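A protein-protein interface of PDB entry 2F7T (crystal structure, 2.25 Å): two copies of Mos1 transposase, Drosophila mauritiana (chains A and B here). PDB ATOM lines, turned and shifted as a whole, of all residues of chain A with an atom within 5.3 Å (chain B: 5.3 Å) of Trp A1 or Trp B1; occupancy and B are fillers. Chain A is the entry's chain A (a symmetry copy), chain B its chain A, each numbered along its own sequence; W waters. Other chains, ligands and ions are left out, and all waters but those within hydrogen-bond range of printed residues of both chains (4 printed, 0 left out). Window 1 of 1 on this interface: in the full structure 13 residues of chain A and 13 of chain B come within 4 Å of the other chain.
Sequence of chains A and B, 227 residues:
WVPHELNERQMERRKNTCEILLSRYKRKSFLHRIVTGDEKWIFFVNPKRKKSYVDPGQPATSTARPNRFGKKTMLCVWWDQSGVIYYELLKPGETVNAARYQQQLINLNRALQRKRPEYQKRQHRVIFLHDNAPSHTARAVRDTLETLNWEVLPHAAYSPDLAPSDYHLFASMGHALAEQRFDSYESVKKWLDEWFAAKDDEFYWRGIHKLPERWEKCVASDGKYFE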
ATOM      1  N   TRP A   1       4.854   6.237 -19.632  1.00  0.00           N
ATOM      2  CA  TRP A   1       3.715   5.424 -20.156  1.00  0.00           C
ATOM      3  C   TRP A   1       2.410   6.234 -20.377  1.00  0.00           C
ATOM      4  O   TRP A   1       2.293   6.960 -21.395  1.00  0.00           O
ATOM      5  CB  TRP A   1       3.463   4.208 -19.261  1.00  0.00           C
ATOM      6  CG  TRP A   1       3.866   2.875 -19.857  1.00  0.00           C
ATOM      7  CD1 TRP A   1       5.066   2.233 -19.689  1.00  0.00           C
ATOM      8  CD2 TRP A   1       3.053   1.994 -20.686  1.00  0.00           C
ATOM      9  NE1 TRP A   1       5.056   1.027 -20.356  1.00  0.00           N
ATOM     10  CE2 TRP A   1       3.840   0.846 -20.975  1.00  0.00           C
ATOM     11  CE3 TRP A   1       1.746   2.063 -21.226  1.00  0.00           C
ATOM     12  CZ2 TRP A   1       3.366  -0.227 -21.775  1.00  0.00           C
ATOM     13  CZ3 TRP A   1       1.276   0.986 -22.014  1.00  0.00           C
ATOM     14  CH2 TRP A   1       2.093  -0.134 -22.279  1.00  0.00           C
ATOM     15  N   VAL A   2       1.453   6.107 -19.437  1.00  0.00           N
ATOM     16  CA  VAL A   2       0.074   6.682 -19.571  1.00  0.00           C
ATOM     17  C   VAL A   2       0.029   8.207 -19.888  1.00  0.00           C
ATOM     18  O   VAL A   2       1.016   8.899 -19.625  1.00  0.00           O
ATOM     19  CB  VAL A   2      -0.854   6.317 -18.363  1.00  0.00           C
ATOM     20  CG1 VAL A   2      -1.576   4.956 -18.611  1.00  0.00           C
ATOM     21  CG2 VAL A   2      -0.086   6.343 -17.061  1.00  0.00           C
ATOM     22  N   PRO A   3      -1.094   8.725 -20.427  1.00  0.00           N
ATOM     23  CA  PRO A   3      -1.049   9.991 -21.204  1.00  0.00           C
ATOM     24  C   PRO A   3      -0.922  11.235 -20.325  1.00  0.00           C
ATOM     25  O   PRO A   3      -1.798  11.467 -19.473  1.00  0.00           O
ATOM     26  CB  PRO A   3      -2.384  10.007 -21.976  1.00  0.00           C
ATOM     27  CG  PRO A   3      -3.267   8.852 -21.370  1.00  0.00           C
ATOM     28  CD  PRO A   3      -2.478   8.214 -20.266  1.00  0.00           C
ATOM     29  N   HIS A   4       0.163  11.999 -20.540  1.00  0.00           N
ATOM     30  CA  HIS A   4       0.454  13.268 -19.847  1.00  0.00           C
ATOM     31  C   HIS A   4      -0.817  14.070 -19.639  1.00  0.00           C
ATOM     32  O   HIS A   4      -1.629  14.256 -20.552  1.00  0.00           O
ATOM     33  CB  HIS A   4       1.476  14.133 -20.631  1.00  0.00           C
ATOM     34  CG  HIS A   4       1.862  15.396 -19.922  1.00  0.00           C
ATOM     35  ND1 HIS A   4       2.992  15.495 -19.132  1.00  0.00           N
ATOM     36  CD2 HIS A   4       1.252  16.606 -19.856  1.00  0.00           C
ATOM     37  CE1 HIS A   4       3.064  16.713 -18.618  1.00  0.00           C
ATOM     38  NE2 HIS A   4       2.017  17.404 -19.037  1.00  0.00           N
ATOM     39  N   TYR A 158       4.361  19.135 -25.369  1.00  0.00           N
ATOM     40  CA  TYR A 158       3.750  17.819 -25.188  1.00  0.00           C
ATOM     41  C   TYR A 158       2.826  17.431 -26.318  1.00  0.00           C
ATOM     42  O   TYR A 158       1.723  16.855 -26.062  1.00  0.00           O
ATOM     43  CB  TYR A 158       2.978  17.853 -23.878  1.00  0.00           C
ATOM     44  CG  TYR A 158       3.874  18.053 -22.685  1.00  0.00           C
ATOM     45  CD1 TYR A 158       3.874  19.263 -21.976  1.00  0.00           C
ATOM     46  CD2 TYR A 158       4.739  17.030 -22.257  1.00  0.00           C
ATOM     47  CE1 TYR A 158       4.728  19.439 -20.853  1.00  0.00           C
ATOM     48  CE2 TYR A 158       5.603  17.203 -21.123  1.00  0.00           C
ATOM     49  CZ  TYR A 158       5.593  18.400 -20.428  1.00  0.00           C
ATOM     50  OH  TYR A 158       6.452  18.595 -19.322  1.00  0.00           O
ATOM     51  N   PRO A 160       3.014  15.394 -29.509  1.00  0.00           N
ATOM     52  CA  PRO A 160       3.382  14.476 -30.509  1.00  0.00           C
ATOM     53  C   PRO A 160       2.224  14.210 -31.435  1.00  0.00           C
ATOM     54  O   PRO A 160       2.421  13.764 -32.588  1.00  0.00           O
ATOM     55  CB  PRO A 160       3.699  13.215 -29.713  1.00  0.00           C
ATOM     56  CG  PRO A 160       2.857  13.297 -28.476  1.00  0.00           C
ATOM     57  CD  PRO A 160       3.042  14.774 -28.166  1.00  0.00           C
ATOM     58  N   ASP A 161       1.031  14.535 -30.982  1.00  0.00           N
ATOM     59  CA  ASP A 161      -0.131  14.426 -31.799  1.00  0.00           C
ATOM     60  C   ASP A 161      -0.148  15.499 -32.865  1.00  0.00           C
ATOM     61  O   ASP A 161      -0.991  15.441 -33.775  1.00  0.00           O
ATOM     62  CB  ASP A 161      -1.398  14.455 -30.916  1.00  0.00           C
ATOM     63  CG  ASP A 161      -1.523  15.694 -30.107  1.00  0.00           C
ATOM     64  OD1 ASP A 161      -2.648  16.067 -29.782  1.00  0.00           O
ATOM     65  OD2 ASP A 161      -0.573  16.402 -29.787  1.00  0.00           O
ATOM     66  N   ASP A 166       5.904  11.798 -35.197  1.00  0.00           N
ATOM     67  CA  ASP A 166       5.440  10.962 -34.130  1.00  0.00           C
ATOM     68  C   ASP A 166       4.134  10.342 -34.528  1.00  0.00           C
ATOM     69  O   ASP A 166       4.054   9.158 -34.538  1.00  0.00           O
ATOM     70  CB  ASP A 166       5.303  11.760 -32.839  1.00  0.00           C
ATOM     71  CG  ASP A 166       6.651  12.329 -32.378  1.00  0.00           C
ATOM     72  OD1 ASP A 166       7.696  11.738 -32.670  1.00  0.00           O
ATOM     73  OD2 ASP A 166       6.813  13.387 -31.790  1.00  0.00           O
ATOM     74  N   TYR A 167       3.118  11.138 -34.898  1.00  0.00           N
ATOM     75  CA  TYR A 167       1.800  10.555 -35.175  1.00  0.00           C
ATOM     76  C   TYR A 167       1.769   9.791 -36.452  1.00  0.00           C
ATOM     77  O   TYR A 167       0.918   8.938 -36.607  1.00  0.00           O
ATOM     78  CB  TYR A 167       0.634  11.591 -35.108  1.00  0.00           C
ATOM     79  CG  TYR A 167       0.607  12.605 -36.234  1.00  0.00           C
ATOM     80  CD1 TYR A 167       0.994  13.953 -36.025  1.00  0.00           C
ATOM     81  CD2 TYR A 167       0.207  12.239 -37.485  1.00  0.00           C
ATOM     82  CE1 TYR A 167       0.955  14.857 -37.083  1.00  0.00           C
ATOM     83  CE2 TYR A 167       0.223  13.147 -38.574  1.00  0.00           C
ATOM     84  CZ  TYR A 167       0.609  14.434 -38.345  1.00  0.00           C
ATOM     85  OH  TYR A 167       0.496  15.326 -39.384  1.00  0.00           O
ATOM     86  N   ARG A 214      -5.559  17.853 -37.900  1.00  0.00           N
ATOM     87  CA  ARG A 214      -5.125  17.788 -36.513  1.00  0.00           C
ATOM     88  C   ARG A 214      -5.144  19.134 -35.835  1.00  0.00           C
ATOM     89  O   ARG A 214      -5.551  19.187 -34.704  1.00  0.00           O
ATOM     90  CB  ARG A 214      -3.767  17.150 -36.391  1.00  0.00           C
ATOM     91  CG  ARG A 214      -3.858  15.746 -36.945  1.00  0.00           C
ATOM     92  CD  ARG A 214      -2.579  15.025 -36.888  1.00  0.00           C
ATOM     93  NE  ARG A 214      -2.930  13.630 -36.795  1.00  0.00           N
ATOM     94  CZ  ARG A 214      -2.883  12.898 -35.687  1.00  0.00           C
ATOM     95  NH1 ARG A 214      -2.429  13.389 -34.540  1.00  0.00           N
ATOM     96  NH2 ARG A 214      -3.230  11.627 -35.776  1.00  0.00           N
ATOM     97  N   TYR A 225      -5.846  16.999 -25.750  1.00  0.00           N
ATOM     98  CA  TYR A 225      -5.597  15.853 -26.617  1.00  0.00           C
ATOM     99  C   TYR A 225      -6.898  15.481 -27.221  1.00  0.00           C
ATOM    100  O   TYR A 225      -7.960  15.833 -26.687  1.00  0.00           O
ATOM    101  CB  TYR A 225      -5.027  14.648 -25.818  1.00  0.00           C
ATOM    102  CG  TYR A 225      -3.596  14.861 -25.405  1.00  0.00           C
ATOM    103  CD1 TYR A 225      -3.211  14.644 -24.107  1.00  0.00           C
ATOM    104  CD2 TYR A 225      -2.638  15.332 -26.314  1.00  0.00           C
ATOM    105  CE1 TYR A 225      -1.900  14.847 -23.683  1.00  0.00           C
ATOM    106  CE2 TYR A 225      -1.259  15.568 -25.893  1.00  0.00           C
ATOM    107  CZ  TYR A 225      -0.934  15.312 -24.567  1.00  0.00           C
ATOM    108  OH  TYR A 225       0.321  15.533 -24.064  1.00  0.00           O
ATOM    109  N   TRP B   1      -1.531  11.291 -24.765  1.00  0.00           N
ATOM    110  CA  TRP B   1      -0.299  10.918 -25.524  1.00  0.00           C
ATOM    111  C   TRP B   1       0.957  10.726 -24.634  1.00  0.00           C
ATOM    112  O   TRP B   1       1.101   9.664 -23.981  1.00  0.00           O
ATOM    113  CB  TRP B   1      -0.031  11.924 -26.646  1.00  0.00           C
ATOM    114  CG  TRP B   1      -0.289  11.411 -28.047  1.00  0.00           C
ATOM    115  CD1 TRP B   1      -1.450  11.544 -28.766  1.00  0.00           C
ATOM    116  CD2 TRP B   1       0.647  10.718 -28.923  1.00  0.00           C
ATOM    117  NE1 TRP B   1      -1.301  10.979 -30.015  1.00  0.00           N
ATOM    118  CE2 TRP B   1      -0.030  10.467 -30.146  1.00  0.00           C
ATOM    119  CE3 TRP B   1       1.984  10.269 -28.792  1.00  0.00           C
ATOM    120  CZ2 TRP B   1       0.581   9.793 -31.237  1.00  0.00           C
ATOM    121  CZ3 TRP B   1       2.590   9.607 -29.886  1.00  0.00           C
ATOM    122  CH2 TRP B   1       1.880   9.376 -31.083  1.00  0.00           C
ATOM    123  N   VAL B   2       1.844  11.740 -24.614  1.00  0.00           N
ATOM    124  CA  VAL B   2       3.185  11.660 -23.946  1.00  0.00           C
ATOM    125  C   VAL B   2       3.144  11.224 -22.450  1.00  0.00           C
ATOM    126  O   VAL B   2       2.092  11.357 -21.819  1.00  0.00           O
ATOM    127  CB  VAL B   2       4.040  12.956 -24.145  1.00  0.00           C
ATOM    128  CG1 VAL B   2       4.875  12.872 -25.460  1.00  0.00           C
ATOM    129  CG2 VAL B   2       3.172  14.193 -24.080  1.00  0.00           C
ATOM    130  N   PRO B   3       4.265  10.727 -21.888  1.00  0.00           N
ATOM    131  CA  PRO B   3       4.190   9.848 -20.692  1.00  0.00           C
ATOM    132  C   PRO B   3       3.906  10.611 -19.398  1.00  0.00           C
ATOM    133  O   PRO B   3       4.693  11.503 -19.035  1.00  0.00           O
ATOM    134  CB  PRO B   3       5.577   9.175 -20.630  1.00  0.00           C
ATOM    135  CG  PRO B   3       6.491   9.936 -21.664  1.00  0.00           C
ATOM    136  CD  PRO B   3       5.666  11.028 -22.276  1.00  0.00           C
ATOM    137  N   HIS B   4       2.789  10.257 -18.740  1.00  0.00           N
ATOM    138  CA  HIS B   4       2.354  10.822 -17.449  1.00  0.00           C
ATOM    139  C   HIS B   4       3.544  11.056 -16.537  1.00  0.00           C
ATOM    140  O   HIS B   4       4.409  10.192 -16.358  1.00  0.00           O
ATOM    141  CB  HIS B   4       1.336   9.899 -16.728  1.00  0.00           C
ATOM    142  CG  HIS B   4       0.806  10.473 -15.449  1.00  0.00           C
ATOM    143  ND1 HIS B   4      -0.386  11.169 -15.379  1.00  0.00           N
ATOM    144  CD2 HIS B   4       1.321  10.484 -14.194  1.00  0.00           C
ATOM    145  CE1 HIS B   4      -0.585  11.576 -14.135  1.00  0.00           C
ATOM    146  NE2 HIS B   4       0.439  11.179 -13.398  1.00  0.00           N
ATOM    147  N   TYR B 158      -1.523   4.574 -12.339  1.00  0.00           N
ATOM    148  CA  TYR B 158      -0.835   4.905 -13.585  1.00  0.00           C
ATOM    149  C   TYR B 158       0.200   3.881 -13.984  1.00  0.00           C
ATOM    150  O   TYR B 158       1.318   4.261 -14.452  1.00  0.00           O
ATOM    151  CB  TYR B 158      -0.172   6.260 -13.392  1.00  0.00           C
ATOM    152  CG  TYR B 158      -1.170   7.365 -13.174  1.00  0.00           C
ATOM    153  CD1 TYR B 158      -1.313   7.973 -11.917  1.00  0.00           C
ATOM    154  CD2 TYR B 158      -1.990   7.812 -14.225  1.00  0.00           C
ATOM    155  CE1 TYR B 158      -2.262   9.012 -11.724  1.00  0.00           C
ATOM    156  CE2 TYR B 158      -2.950   8.863 -14.035  1.00  0.00           C
ATOM    157  CZ  TYR B 158      -3.081   9.457 -12.792  1.00  0.00           C
ATOM    158  OH  TYR B 158      -4.035  10.478 -12.581  1.00  0.00           O
ATOM    159  N   PRO B 160       0.409   0.860 -16.266  1.00  0.00           N
ATOM    160  CA  PRO B 160       0.187  -0.086 -17.282  1.00  0.00           C
ATOM    161  C   PRO B 160       1.429  -0.901 -17.527  1.00  0.00           C
ATOM    162  O   PRO B 160       1.355  -2.025 -18.072  1.00  0.00           O
ATOM    163  CB  PRO B 160      -0.100   0.786 -18.501  1.00  0.00           C
ATOM    164  CG  PRO B 160       0.635   2.068 -18.260  1.00  0.00           C
ATOM    165  CD  PRO B 160       0.321   2.244 -16.783  1.00  0.00           C
ATOM    166  N   ASP B 161       2.556  -0.392 -17.076  1.00  0.00           N
ATOM    167  CA  ASP B 161       3.784  -1.111 -17.157  1.00  0.00           C
ATOM    168  C   ASP B 161       3.807  -2.257 -16.168  1.00  0.00           C
ATOM    169  O   ASP B 161       4.720  -3.096 -16.229  1.00  0.00           O
ATOM    170  CB  ASP B 161       4.973  -0.144 -16.962  1.00  0.00           C
ATOM    171  CG  ASP B 161       4.944   0.568 -15.659  1.00  0.00           C
ATOM    172  OD1 ASP B 161       6.011   0.942 -15.176  1.00  0.00           O
ATOM    173  OD2 ASP B 161       3.924   0.760 -15.006  1.00  0.00           O
ATOM    174  N   ASP B 166      -1.763  -4.710 -20.496  1.00  0.00           N
ATOM    175  CA  ASP B 166      -1.324  -3.548 -21.210  1.00  0.00           C
ATOM    176  C   ASP B 166       0.049  -3.799 -21.754  1.00  0.00           C
ATOM    177  O   ASP B 166       0.215  -3.707 -22.926  1.00  0.00           O
ATOM    178  CB  ASP B 166      -1.346  -2.320 -20.309  1.00  0.00           C
ATOM    179  CG  ASP B 166      -2.764  -2.005 -19.813  1.00  0.00           C
ATOM    180  OD1 ASP B 166      -3.737  -2.322 -20.504  1.00  0.00           O
ATOM    181  OD2 ASP B 166      -3.046  -1.518 -18.730  1.00  0.00           O
ATOM    182  N   TYR B 167       1.032  -4.159 -20.913  1.00  0.00           N
ATOM    183  CA  TYR B 167       2.406  -4.292 -21.410  1.00  0.00           C
ATOM    184  C   TYR B 167       2.591  -5.497 -22.264  1.00  0.00           C
ATOM    185  O   TYR B 167       3.511  -5.520 -23.057  1.00  0.00           O
ATOM    186  CB  TYR B 167       3.486  -4.225 -20.285  1.00  0.00           C
ATOM    187  CG  TYR B 167       3.527  -5.425 -19.360  1.00  0.00           C
ATOM    188  CD1 TYR B 167       3.029  -5.355 -18.033  1.00  0.00           C
ATOM    189  CD2 TYR B 167       4.048  -6.610 -19.786  1.00  0.00           C
ATOM    190  CE1 TYR B 167       3.085  -6.477 -17.212  1.00  0.00           C
ATOM    191  CE2 TYR B 167       4.052  -7.767 -18.968  1.00  0.00           C
ATOM    192  CZ  TYR B 167       3.558  -7.672 -17.701  1.00  0.00           C
ATOM    193  OH  TYR B 167       3.687  -8.769 -16.884  1.00  0.00           O
ATOM    194  N   ARG B 214       9.410  -7.063 -13.788  1.00  0.00           N
ATOM    195  CA  ARG B 214       8.875  -5.710 -13.781  1.00  0.00           C
ATOM    196  C   ARG B 214       8.744  -5.145 -12.391  1.00  0.00           C
ATOM    197  O   ARG B 214       9.056  -3.996 -12.221  1.00  0.00           O
ATOM    198  CB  ARG B 214       7.561  -5.635 -14.513  1.00  0.00           C
ATOM    199  CG  ARG B 214       7.796  -6.065 -15.943  1.00  0.00           C
ATOM    200  CD  ARG B 214       6.571  -6.043 -16.755  1.00  0.00           C
ATOM    201  NE  ARG B 214       7.014  -5.811 -18.108  1.00  0.00           N
ATOM    202  CZ  ARG B 214       6.934  -4.654 -18.754  1.00  0.00           C
ATOM    203  NH1 ARG B 214       6.357  -3.586 -18.215  1.00  0.00           N
ATOM    204  NH2 ARG B 214       7.377  -4.614 -19.998  1.00  0.00           N
ATOM    205  N   TYR B 225       8.810   5.105 -13.695  1.00  0.00           N
ATOM    206  CA  TYR B 225       8.712   4.318 -14.920  1.00  0.00           C
ATOM    207  C   TYR B 225      10.079   3.842 -15.234  1.00  0.00           C
ATOM    208  O   TYR B 225      11.069   4.421 -14.760  1.00  0.00           O
ATOM    209  CB  TYR B 225       8.170   5.169 -16.102  1.00  0.00           C
ATOM    210  CG  TYR B 225       6.700   5.459 -15.969  1.00  0.00           C
ATOM    211  CD1 TYR B 225       6.231   6.739 -16.118  1.00  0.00           C
ATOM    212  CD2 TYR B 225       5.784   4.449 -15.645  1.00  0.00           C
ATOM    213  CE1 TYR B 225       4.880   7.050 -15.986  1.00  0.00           C
ATOM    214  CE2 TYR B 225       4.362   4.749 -15.486  1.00  0.00           C
ATOM    215  CZ  TYR B 225       3.954   6.064 -15.666  1.00  0.00           C
ATOM    216  OH  TYR B 225       2.651   6.456 -15.506  1.00  0.00           O
HETATM  217  O   HOH W   1      -0.018   7.382 -23.353  1.00  0.00           O
HETATM  218  O   HOH W   2       3.520   7.849 -23.528  1.00  0.00           O
HETATM  219  O   HOH W   3      -2.170  10.983 -32.333  1.00  0.00           O
HETATM  220  O   HOH W   4       6.101  -1.215 -20.461  1.00  0.00           O
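Of chain B, only Trp B1, Pro B3, Pro B160, Asp B161 and Tyr B225 come within 4 Å of Trp A1.
Of the printed residues of chain B, His A4 touches Val B2 (2.4 Å) and His B4 (3.6 Å).
Trp B1 touches just these residues of chain A: Trp A1, Pro A3, Pro A160, Asp A161 and Tyr A225.
Of the printed residues of chain A, Tyr B158 touches Val A2.
The nearest residue of chain B that does not touch Trp A1 is Asp B166 (4.1 Å).
The nearest residue of chain A that does not touch Trp B1 is Asp A166 (4.1 Å).
The nearest printed residue of chain B that does not touch His A4 is Pro B3 (4.2 Å).
The backbone carbonyl oxygen (O) of Val B2 sits at hydrogen-bond distance from the backbone NH (N) of His A4.
The backbone carbonyl oxygen (O) of Val A2 sits at hydrogen-bond distance from the backbone NH (N) of His B4.
The backbone carbonyl oxygen (O) of Val B2 sits close to the backbone carbonyl oxygen (O) of Val A2 (3.5 Å).
Among the printed residues, pairs that only touch across the chains: Val A2 with Tyr B225, Tyr A225 with Val B2, Pro A160 with Trp B1, Trp A1 with Pro B160, Trp A1 with Pro B3, Pro A3 with Trp B1, Pro A3 with Val B2, Val A2 with Pro B3, Trp A1 with Asp B161, Asp A161 with Trp B1, Val A2 with Tyr B158, Tyr A158 with Val B2, His A4 with His B4, Pro A160 with Val B2, Val A2 with Pro B160, Tyr A225 with Trp B1, Trp A1 with Tyr B225 and Trp A1 with Trp B1.
Water W4 lies within hydrogen-bond range of NE1 of Trp A1 (2.5 Å) and NH1 of Arg B214 (3.3 Å).
Water W3 bridges the indole nitrogen (NE1) of Trp B1 and the guanidinium group (NH1) of Arg A214.
Water W1 lies within hydrogen-bond range of the backbone carbonyl oxygen of Trp B1 (2.6 Å) and the backbone carbonyl oxygen of Trp A1 (3.1 Å).
Water W2 bridges O of Trp A1 (2.6 Å) and O of Trp B1 (3.1 Å).
Trp A1 touches Pro B3, and with the chains exchanged Pro A3 touches Trp B1.
Val A2 touches His B4, and with the chains exchanged His A4 touches Val B2.
Val A2 touches Pro B160, and with the chains exchanged Pro A160 touches Val B2.
Val A2 touches Tyr B225, and with the chains exchanged Tyr A225 touches Val B2.
Positions printed for both chains: 1, 2, 3, 4, 158, 160, 161, 166, 167, 214 and 225.
Of the 11 printed residues of chain B, 8 touch a printed residue of chain A.
Hydrophobic or aromatic side chains of chain B within 4 Å of the printed part of chain A: Trp B1, Val B2, Pro B3, His B4, Tyr B158, Pro B160 and Tyr B225.
Among the printed residues, 21 pairs touch across the chains.
The backbone carbonyl oxygen (O) of Tyr B158 is in hydrogen-bond range of the side-chain hydroxyl (OH) of Tyr B225, 2.8 Å away.
The guanidinium group of Arg B214 is in hydrogen-bond range of the backbone carbonyl oxygen of Asp B161 (2.6 Å).
O of Tyr A158 is in hydrogen-bond range of OH of Tyr A225 (2.8 Å).
The backbone carbonyl oxygen (O) of Asp A161 is in hydrogen-bond range of the guanidinium group (NH1) of Arg A214.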
